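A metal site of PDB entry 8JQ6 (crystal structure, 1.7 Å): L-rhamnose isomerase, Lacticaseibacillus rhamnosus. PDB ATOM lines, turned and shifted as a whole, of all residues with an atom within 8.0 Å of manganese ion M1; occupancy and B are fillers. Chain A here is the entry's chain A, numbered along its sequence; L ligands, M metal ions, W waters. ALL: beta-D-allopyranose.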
ATOM      1  N   TRP A 187     -26.426 -29.938  17.479  1.00  0.00           N
ATOM      2  CA  TRP A 187     -24.960 -29.956  17.676  1.00  0.00           C
ATOM      3  C   TRP A 187     -24.343 -31.009  16.767  1.00  0.00           C
ATOM      4  O   TRP A 187     -24.799 -32.156  16.790  1.00  0.00           O
ATOM      5  CB  TRP A 187     -24.555 -30.174  19.141  1.00  0.00           C
ATOM      6  CG  TRP A 187     -23.064 -30.260  19.223  1.00  0.00           C
ATOM      7  CD1 TRP A 187     -22.182 -29.225  19.067  1.00  0.00           C
ATOM      8  CD2 TRP A 187     -22.271 -31.455  19.294  1.00  0.00           C
ATOM      9  NE1 TRP A 187     -20.895 -29.697  19.061  1.00  0.00           N
ATOM     10  CE2 TRP A 187     -20.922 -31.065  19.229  1.00  0.00           C
ATOM     11  CE3 TRP A 187     -22.564 -32.816  19.448  1.00  0.00           C
ATOM     12  CZ2 TRP A 187     -19.868 -31.973  19.315  1.00  0.00           C
ATOM     13  CZ3 TRP A 187     -21.528 -33.723  19.547  1.00  0.00           C
ATOM     14  CH2 TRP A 187     -20.202 -33.306  19.469  1.00  0.00           C
ATOM     15  N   GLU A 228     -25.882 -24.985  17.821  1.00  0.00           N
ATOM     16  CA  GLU A 228     -24.854 -24.987  18.885  1.00  0.00           C
ATOM     17  C   GLU A 228     -23.468 -25.136  18.260  1.00  0.00           C
ATOM     18  O   GLU A 228     -23.162 -26.218  17.735  1.00  0.00           O
ATOM     19  CB  GLU A 228     -25.120 -26.130  19.865  1.00  0.00           C
ATOM     20  CG  GLU A 228     -24.047 -26.249  20.922  1.00  0.00           C
ATOM     21  CD  GLU A 228     -24.340 -27.261  22.015  1.00  0.00           C
ATOM     22  OE1 GLU A 228     -25.304 -28.039  21.870  1.00  0.00           O
ATOM     23  OE2 GLU A 228     -23.615 -27.251  23.004  1.00  0.00           O
ATOM     24  N   GLY A 229     -22.656 -24.081  18.350  1.00  0.00           N
ATOM     25  CA  GLY A 229     -21.250 -24.083  17.924  1.00  0.00           C
ATOM     26  C   GLY A 229     -20.326 -24.633  19.005  1.00  0.00           C
ATOM     27  O   GLY A 229     -20.753 -24.814  20.178  1.00  0.00           O
ATOM     28  N   LYS A 230     -19.087 -24.879  18.627  1.00  0.00           N
ATOM     29  CA  LYS A 230     -18.035 -25.381  19.533  1.00  0.00           C
ATOM     30  C   LYS A 230     -16.710 -24.857  18.999  1.00  0.00           C
ATOM     31  O   LYS A 230     -16.617 -24.662  17.785  1.00  0.00           O
ATOM     32  CB  LYS A 230     -18.108 -26.911  19.540  1.00  0.00           C
ATOM     33  CG  LYS A 230     -17.349 -27.600  20.651  1.00  0.00           C
ATOM     34  CD  LYS A 230     -17.717 -29.061  20.761  1.00  0.00           C
ATOM     35  CE  LYS A 230     -17.112 -29.743  21.956  1.00  0.00           C
ATOM     36  NZ  LYS A 230     -17.562 -31.153  22.039  1.00  0.00           N
ATOM     37  N   PHE A 232     -13.582 -26.437  19.891  1.00  0.00           N
ATOM     38  CA  PHE A 232     -12.776 -27.680  19.684  1.00  0.00           C
ATOM     39  C   PHE A 232     -13.305 -28.806  20.562  1.00  0.00           C
ATOM     40  O   PHE A 232     -13.857 -28.563  21.635  1.00  0.00           O
ATOM     41  CB  PHE A 232     -11.312 -27.424  20.000  1.00  0.00           C
ATOM     42  CG  PHE A 232     -10.974 -27.377  21.474  1.00  0.00           C
ATOM     43  CD1 PHE A 232     -10.394 -28.475  22.093  1.00  0.00           C
ATOM     44  CD2 PHE A 232     -11.234 -26.248  22.223  1.00  0.00           C
ATOM     45  CE1 PHE A 232     -10.067 -28.426  23.436  1.00  0.00           C
ATOM     46  CE2 PHE A 232     -10.901 -26.201  23.574  1.00  0.00           C
ATOM     47  CZ  PHE A 232     -10.332 -27.293  24.177  1.00  0.00           C
ATOM     48  N   ASP A 261     -23.106 -22.566  24.583  1.00  0.00           N
ATOM     49  CA  ASP A 261     -22.682 -23.522  25.636  1.00  0.00           C
ATOM     50  C   ASP A 261     -21.441 -22.943  26.317  1.00  0.00           C
ATOM     51  O   ASP A 261     -20.447 -22.702  25.628  1.00  0.00           O
ATOM     52  CB  ASP A 261     -22.473 -24.932  25.069  1.00  0.00           C
ATOM     53  CG  ASP A 261     -22.055 -25.920  26.128  1.00  0.00           C
ATOM     54  OD1 ASP A 261     -22.664 -27.006  26.191  1.00  0.00           O
ATOM     55  OD2 ASP A 261     -21.127 -25.605  26.889  1.00  0.00           O
ATOM     56  N   ALA A 262     -21.547 -22.691  27.626  1.00  0.00           N
ATOM     57  CA  ALA A 262     -20.548 -21.944  28.431  1.00  0.00           C
ATOM     58  C   ALA A 262     -19.213 -22.697  28.461  1.00  0.00           C
ATOM     59  O   ALA A 262     -18.215 -22.089  28.865  1.00  0.00           O
ATOM     60  CB  ALA A 262     -21.084 -21.742  29.821  1.00  0.00           C
ATOM     61  N   GLY A 263     -19.182 -23.958  28.017  1.00  0.00           N
ATOM     62  CA  GLY A 263     -17.948 -24.779  28.032  1.00  0.00           C
ATOM     63  C   GLY A 263     -17.191 -24.756  26.715  1.00  0.00           C
ATOM     64  O   GLY A 263     -16.099 -25.347  26.640  1.00  0.00           O
ATOM     65  N   HIS A 264     -17.711 -24.085  25.684  1.00  0.00           N
ATOM     66  CA  HIS A 264     -17.277 -24.329  24.275  1.00  0.00           C
ATOM     67  C   HIS A 264     -16.504 -23.132  23.706  1.00  0.00           C
ATOM     68  O   HIS A 264     -16.352 -23.090  22.463  1.00  0.00           O
ATOM     69  CB  HIS A 264     -18.495 -24.658  23.409  1.00  0.00           C
ATOM     70  CG  HIS A 264     -19.132 -25.968  23.731  1.00  0.00           C
ATOM     71  ND1 HIS A 264     -20.097 -26.519  22.930  1.00  0.00           N
ATOM     72  CD2 HIS A 264     -18.922 -26.847  24.732  1.00  0.00           C
ATOM     73  CE1 HIS A 264     -20.487 -27.668  23.438  1.00  0.00           C
ATOM     74  NE2 HIS A 264     -19.771 -27.904  24.541  1.00  0.00           N
ATOM     75  N   HIS A 288     -26.774 -22.920  27.278  1.00  0.00           N
ATOM     76  CA  HIS A 288     -26.339 -24.199  27.899  1.00  0.00           C
ATOM     77  C   HIS A 288     -25.297 -23.904  28.977  1.00  0.00           C
ATOM     78  O   HIS A 288     -24.132 -23.674  28.608  1.00  0.00           O
ATOM     79  CB  HIS A 288     -25.725 -25.167  26.881  1.00  0.00           C
ATOM     80  CG  HIS A 288     -26.719 -25.982  26.138  1.00  0.00           C
ATOM     81  ND1 HIS A 288     -26.333 -27.087  25.398  1.00  0.00           N
ATOM     82  CD2 HIS A 288     -28.058 -25.861  26.001  1.00  0.00           C
ATOM     83  CE1 HIS A 288     -27.407 -27.628  24.842  1.00  0.00           C
ATOM     84  NE2 HIS A 288     -28.470 -26.885  25.187  1.00  0.00           N
ATOM     85  N   VAL A 289     -25.693 -23.923  30.246  1.00  0.00           N
ATOM     86  CA  VAL A 289     -24.736 -23.737  31.361  1.00  0.00           C
ATOM     87  C   VAL A 289     -24.021 -25.079  31.576  1.00  0.00           C
ATOM     88  O   VAL A 289     -24.671 -26.141  31.611  1.00  0.00           O
ATOM     89  CB  VAL A 289     -25.383 -23.159  32.638  1.00  0.00           C
ATOM     90  CG1 VAL A 289     -25.892 -21.754  32.401  1.00  0.00           C
ATOM     91  CG2 VAL A 289     -26.495 -24.033  33.185  1.00  0.00           C
ATOM     92  N   SER A 290     -22.696 -24.996  31.627  1.00  0.00           N
ATOM     93  CA  SER A 290     -21.747 -26.121  31.651  1.00  0.00           C
ATOM     94  C   SER A 290     -20.436 -25.570  32.210  1.00  0.00           C
ATOM     95  O   SER A 290     -20.148 -24.407  31.918  1.00  0.00           O
ATOM     96  CB  SER A 290     -21.564 -26.679  30.262  1.00  0.00           C
ATOM     97  OG  SER A 290     -20.845 -27.900  30.312  1.00  0.00           O
ATOM     98  N   ARG A 291     -19.700 -26.350  32.991  1.00  0.00           N
ATOM     99  CA  ARG A 291     -18.416 -25.877  33.555  1.00  0.00           C
ATOM    100  C   ARG A 291     -17.263 -26.542  32.806  1.00  0.00           C
ATOM    101  O   ARG A 291     -17.045 -27.741  32.936  1.00  0.00           O
ATOM    102  CB  ARG A 291     -18.304 -26.183  35.057  1.00  0.00           C
ATOM    103  CG  ARG A 291     -16.923 -25.873  35.625  1.00  0.00           C
ATOM    104  CD  ARG A 291     -16.933 -25.804  37.135  1.00  0.00           C
ATOM    105  NE  ARG A 291     -17.603 -26.963  37.696  1.00  0.00           N
ATOM    106  CZ  ARG A 291     -17.046 -27.832  38.533  1.00  0.00           C
ATOM    107  NH1 ARG A 291     -17.743 -28.869  38.963  1.00  0.00           N
ATOM    108  NH2 ARG A 291     -15.801 -27.687  38.914  1.00  0.00           N
ATOM    109  N   PRO A 292     -16.490 -25.763  32.022  1.00  0.00           N
ATOM    110  CA  PRO A 292     -15.257 -26.265  31.436  1.00  0.00           C
ATOM    111  C   PRO A 292     -14.109 -26.137  32.448  1.00  0.00           C
ATOM    112  O   PRO A 292     -13.942 -25.078  33.014  1.00  0.00           O
ATOM    113  CB  PRO A 292     -15.028 -25.318  30.265  1.00  0.00           C
ATOM    114  CG  PRO A 292     -15.567 -23.995  30.781  1.00  0.00           C
ATOM    115  CD  PRO A 292     -16.740 -24.353  31.682  1.00  0.00           C
ATOM    116  N   TRP A 295     -10.712 -27.460  29.394  1.00  0.00           N
ATOM    117  CA  TRP A 295     -11.247 -27.923  28.083  1.00  0.00           C
ATOM    118  C   TRP A 295     -12.751 -28.090  28.216  1.00  0.00           C
ATOM    119  O   TRP A 295     -13.293 -27.804  29.297  1.00  0.00           O
ATOM    120  CB  TRP A 295     -10.526 -29.203  27.619  1.00  0.00           C
ATOM    121  CG  TRP A 295     -10.905 -30.465  28.334  1.00  0.00           C
ATOM    122  CD1 TRP A 295     -10.585 -30.822  29.610  1.00  0.00           C
ATOM    123  CD2 TRP A 295     -11.673 -31.574  27.803  1.00  0.00           C
ATOM    124  NE1 TRP A 295     -11.090 -32.069  29.899  1.00  0.00           N
ATOM    125  CE2 TRP A 295     -11.762 -32.541  28.819  1.00  0.00           C
ATOM    126  CE3 TRP A 295     -12.287 -31.827  26.567  1.00  0.00           C
ATOM    127  CZ2 TRP A 295     -12.461 -33.745  28.639  1.00  0.00           C
ATOM    128  CZ3 TRP A 295     -12.976 -33.012  26.398  1.00  0.00           C
ATOM    129  CH2 TRP A 295     -13.060 -33.958  27.418  1.00  0.00           C
ATOM    130  N   ASP A 296     -13.418 -28.527  27.145  1.00  0.00           N
ATOM    131  CA  ASP A 296     -14.873 -28.826  27.175  1.00  0.00           C
ATOM    132  C   ASP A 296     -15.097 -30.122  27.960  1.00  0.00           C
ATOM    133  O   ASP A 296     -15.413 -31.150  27.330  1.00  0.00           O
ATOM    134  CB  ASP A 296     -15.443 -28.962  25.769  1.00  0.00           C
ATOM    135  CG  ASP A 296     -16.926 -29.268  25.791  1.00  0.00           C
ATOM    136  OD1 ASP A 296     -17.595 -28.795  26.733  1.00  0.00           O
ATOM    137  OD2 ASP A 296     -17.389 -29.991  24.887  1.00  0.00           O
ATOM    138  N   SER A 297     -14.967 -30.039  29.288  1.00  0.00           N
ATOM    139  CA  SER A 297     -14.896 -31.199  30.216  1.00  0.00           C
ATOM    140  C   SER A 297     -16.289 -31.581  30.744  1.00  0.00           C
ATOM    141  O   SER A 297     -16.424 -32.675  31.320  1.00  0.00           O
ATOM    142  CB  SER A 297     -13.961 -30.910  31.355  1.00  0.00           C
ATOM    143  OG  SER A 297     -14.341 -29.721  32.030  1.00  0.00           O
ATOM    144  N   ASP A 298     -17.269 -30.698  30.573  1.00  0.00           N
ATOM    145  CA  ASP A 298     -18.676 -30.971  30.945  1.00  0.00           C
ATOM    146  C   ASP A 298     -18.785 -31.273  32.450  1.00  0.00           C
ATOM    147  O   ASP A 298     -19.577 -32.154  32.834  1.00  0.00           O
ATOM    148  CB  ASP A 298     -19.237 -32.076  30.044  1.00  0.00           C
ATOM    149  CG  ASP A 298     -19.340 -31.597  28.606  1.00  0.00           C
ATOM    150  OD1 ASP A 298     -19.584 -30.401  28.418  1.00  0.00           O
ATOM    151  OD2 ASP A 298     -19.146 -32.402  27.684  1.00  0.00           O
ATOM    152  N   HIS A 299     -18.017 -30.571  33.287  1.00  0.00           N
ATOM    153  CA  HIS A 299     -18.174 -30.602  34.764  1.00  0.00           C
ATOM    154  C   HIS A 299     -19.544 -30.058  35.156  1.00  0.00           C
ATOM    155  O   HIS A 299     -20.122 -29.221  34.424  1.00  0.00           O
ATOM    156  CB  HIS A 299     -17.068 -29.807  35.473  1.00  0.00           C
ATOM    157  CG  HIS A 299     -15.760 -30.531  35.582  1.00  0.00           C
ATOM    158  ND1 HIS A 299     -14.979 -30.824  34.471  1.00  0.00           N
ATOM    159  CD2 HIS A 299     -15.104 -31.009  36.659  1.00  0.00           C
ATOM    160  CE1 HIS A 299     -13.873 -31.432  34.874  1.00  0.00           C
ATOM    161  NE2 HIS A 299     -13.944 -31.577  36.203  1.00  0.00           N
ATOM    162  N   ASP A 328     -26.118 -28.539  30.642  1.00  0.00           N
ATOM    163  CA  ASP A 328     -25.363 -29.526  29.836  1.00  0.00           C
ATOM    164  C   ASP A 328     -24.066 -29.867  30.562  1.00  0.00           C
ATOM    165  O   ASP A 328     -23.134 -29.045  30.604  1.00  0.00           O
ATOM    166  CB  ASP A 328     -25.108 -29.044  28.416  1.00  0.00           C
ATOM    167  CG  ASP A 328     -24.599 -30.168  27.520  1.00  0.00           C
ATOM    168  OD1 ASP A 328     -24.337 -29.899  26.352  1.00  0.00           O
ATOM    169  OD2 ASP A 328     -24.475 -31.302  28.015  1.00  0.00           O
ATOM    170  N   PHE A 329     -24.012 -31.066  31.122  1.00  0.00           N
ATOM    171  CA  PHE A 329     -22.805 -31.572  31.792  1.00  0.00           C
ATOM    172  C   PHE A 329     -22.942 -33.076  31.928  1.00  0.00           C
ATOM    173  O   PHE A 329     -24.045 -33.620  31.744  1.00  0.00           O
ATOM    174  CB  PHE A 329     -22.557 -30.875  33.129  1.00  0.00           C
ATOM    175  CG  PHE A 329     -23.717 -30.795  34.092  1.00  0.00           C
ATOM    176  CD1 PHE A 329     -24.102 -31.903  34.837  1.00  0.00           C
ATOM    177  CD2 PHE A 329     -24.372 -29.604  34.316  1.00  0.00           C
ATOM    178  CE1 PHE A 329     -25.140 -31.815  35.755  1.00  0.00           C
ATOM    179  CE2 PHE A 329     -25.416 -29.514  35.225  1.00  0.00           C
ATOM    180  CZ  PHE A 329     -25.799 -30.626  35.943  1.00  0.00           C
ATOM    181  N   PHE A 330     -21.828 -33.735  32.182  1.00  0.00           N
ATOM    182  CA  PHE A 330     -21.757 -35.203  32.286  1.00  0.00           C
ATOM    183  C   PHE A 330     -20.632 -35.540  33.247  1.00  0.00           C
ATOM    184  O   PHE A 330     -19.458 -35.412  32.888  1.00  0.00           O
ATOM    185  CB  PHE A 330     -21.589 -35.826  30.886  1.00  0.00           C
ATOM    186  CG  PHE A 330     -21.285 -37.299  30.952  1.00  0.00           C
ATOM    187  CD1 PHE A 330     -20.367 -37.880  30.091  1.00  0.00           C
ATOM    188  CD2 PHE A 330     -21.885 -38.096  31.914  1.00  0.00           C
ATOM    189  CE1 PHE A 330     -20.084 -39.239  30.173  1.00  0.00           C
ATOM    190  CE2 PHE A 330     -21.592 -39.450  32.002  1.00  0.00           C
ATOM    191  CZ  PHE A 330     -20.685 -40.013  31.130  1.00  0.00           C
HETATM  192  C1  ALL L   1     -21.347 -32.875  23.763  1.00  0.00           C
HETATM  193  C2  ALL L   1     -21.217 -31.671  22.823  1.00  0.00           C
HETATM  194  C3  ALL L   1     -22.302 -30.611  23.062  1.00  0.00           C
HETATM  195  C4  ALL L   1     -23.706 -31.258  23.118  1.00  0.00           C
HETATM  196  C5  ALL L   1     -23.694 -32.456  24.100  1.00  0.00           C
HETATM  197  C6  ALL L   1     -25.025 -33.190  24.138  1.00  0.00           C
HETATM  198  O1  ALL L   1     -20.433 -33.917  23.333  1.00  0.00           O
HETATM  199  O2  ALL L   1     -19.944 -31.060  23.012  1.00  0.00           O
HETATM  200  O3  ALL L   1     -21.979 -29.932  24.291  1.00  0.00           O
HETATM  201  O4  ALL L   1     -24.746 -30.301  23.456  1.00  0.00           O
HETATM  202  O5  ALL L   1     -22.682 -33.397  23.736  1.00  0.00           O
HETATM  203  O6  ALL L   1     -25.670 -33.136  22.861  1.00  0.00           O
HETATM  204 MN    MN M   1     -19.488 -29.307  26.505  1.00  0.00          MN
HETATM  205 MN    MN M   2     -24.116 -28.155  24.922  1.00  0.00          MN
HETATM  206  O   HOH W   1     -19.651 -30.815  25.254  1.00  0.00           O
HETATM  207  O   HOH W   2     -21.532 -29.352  26.727  1.00  0.00           O
HETATM  208  O   HOH W   3     -19.840 -27.533  27.950  1.00  0.00           O
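O3 of the ligand sits close to NE2 of His 264 (3.0 Å).
The side-chain carboxylate of Asp 296 lies within hydrogen-bond range of an oxygen (O2) of the ligand (3.3 Å).
NZ of Lys 230 lies within hydrogen-bond range of O2 of the ligand, 2.6 Å away.
The side-chain carboxylate (OD2) of Asp 296 is in salt-bridge range of the side-chain amino group (NZ) of Lys 230.
ND1 of His 264 is in hydrogen-bond range of O of Gly 229 (3.3 Å).
The backbone carbonyl oxygen (O) of Asp 298 is in hydrogen-bond range of the backbone NH (N) of Phe 330, at 2.8 Å.
The backbone NH of Gly 263 sits at hydrogen-bond distance from the side-chain carboxylate of Asp 261 (2.8 Å).
The side-chain carboxylate (OD1) of Asp 298 lies close to the side-chain hydroxyl (OG) of Ser 290, 3.4 Å away.
Merely in contact with manganese ion M1: Asp 261.
Four residues have an atom within 4 Å of manganese ion M1: Asp 261, His 264, Asp 296 and Asp 298.
Manganese ion M1 is bound by water W1.
Manganese ion M1 is bound by OD1 of Asp 296 (2.0 Å).
Water W2 is bound to manganese ion M1 (2.1 Å).
Manganese ion M1 is bound by OD1 of Asp 298, 2.2 Å away.
Manganese ion M1 is bound by water W3 (2.3 Å).
NE2 of His 264 binds manganese ion M1, 2.4 Å away.
Manganese ion M1 has six donor atoms within binding distance.
Slightly farther from manganese ion M1 lies OD2 of Asp 296 (2.7 Å).
Water W3 lies within hydrogen-bond range of OD2 of Asp 261 and OG of Ser 290.
Water W1 lies within hydrogen-bond range of OD2 of Asp 296, O3 of the ligand and OD2 of Asp 298.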
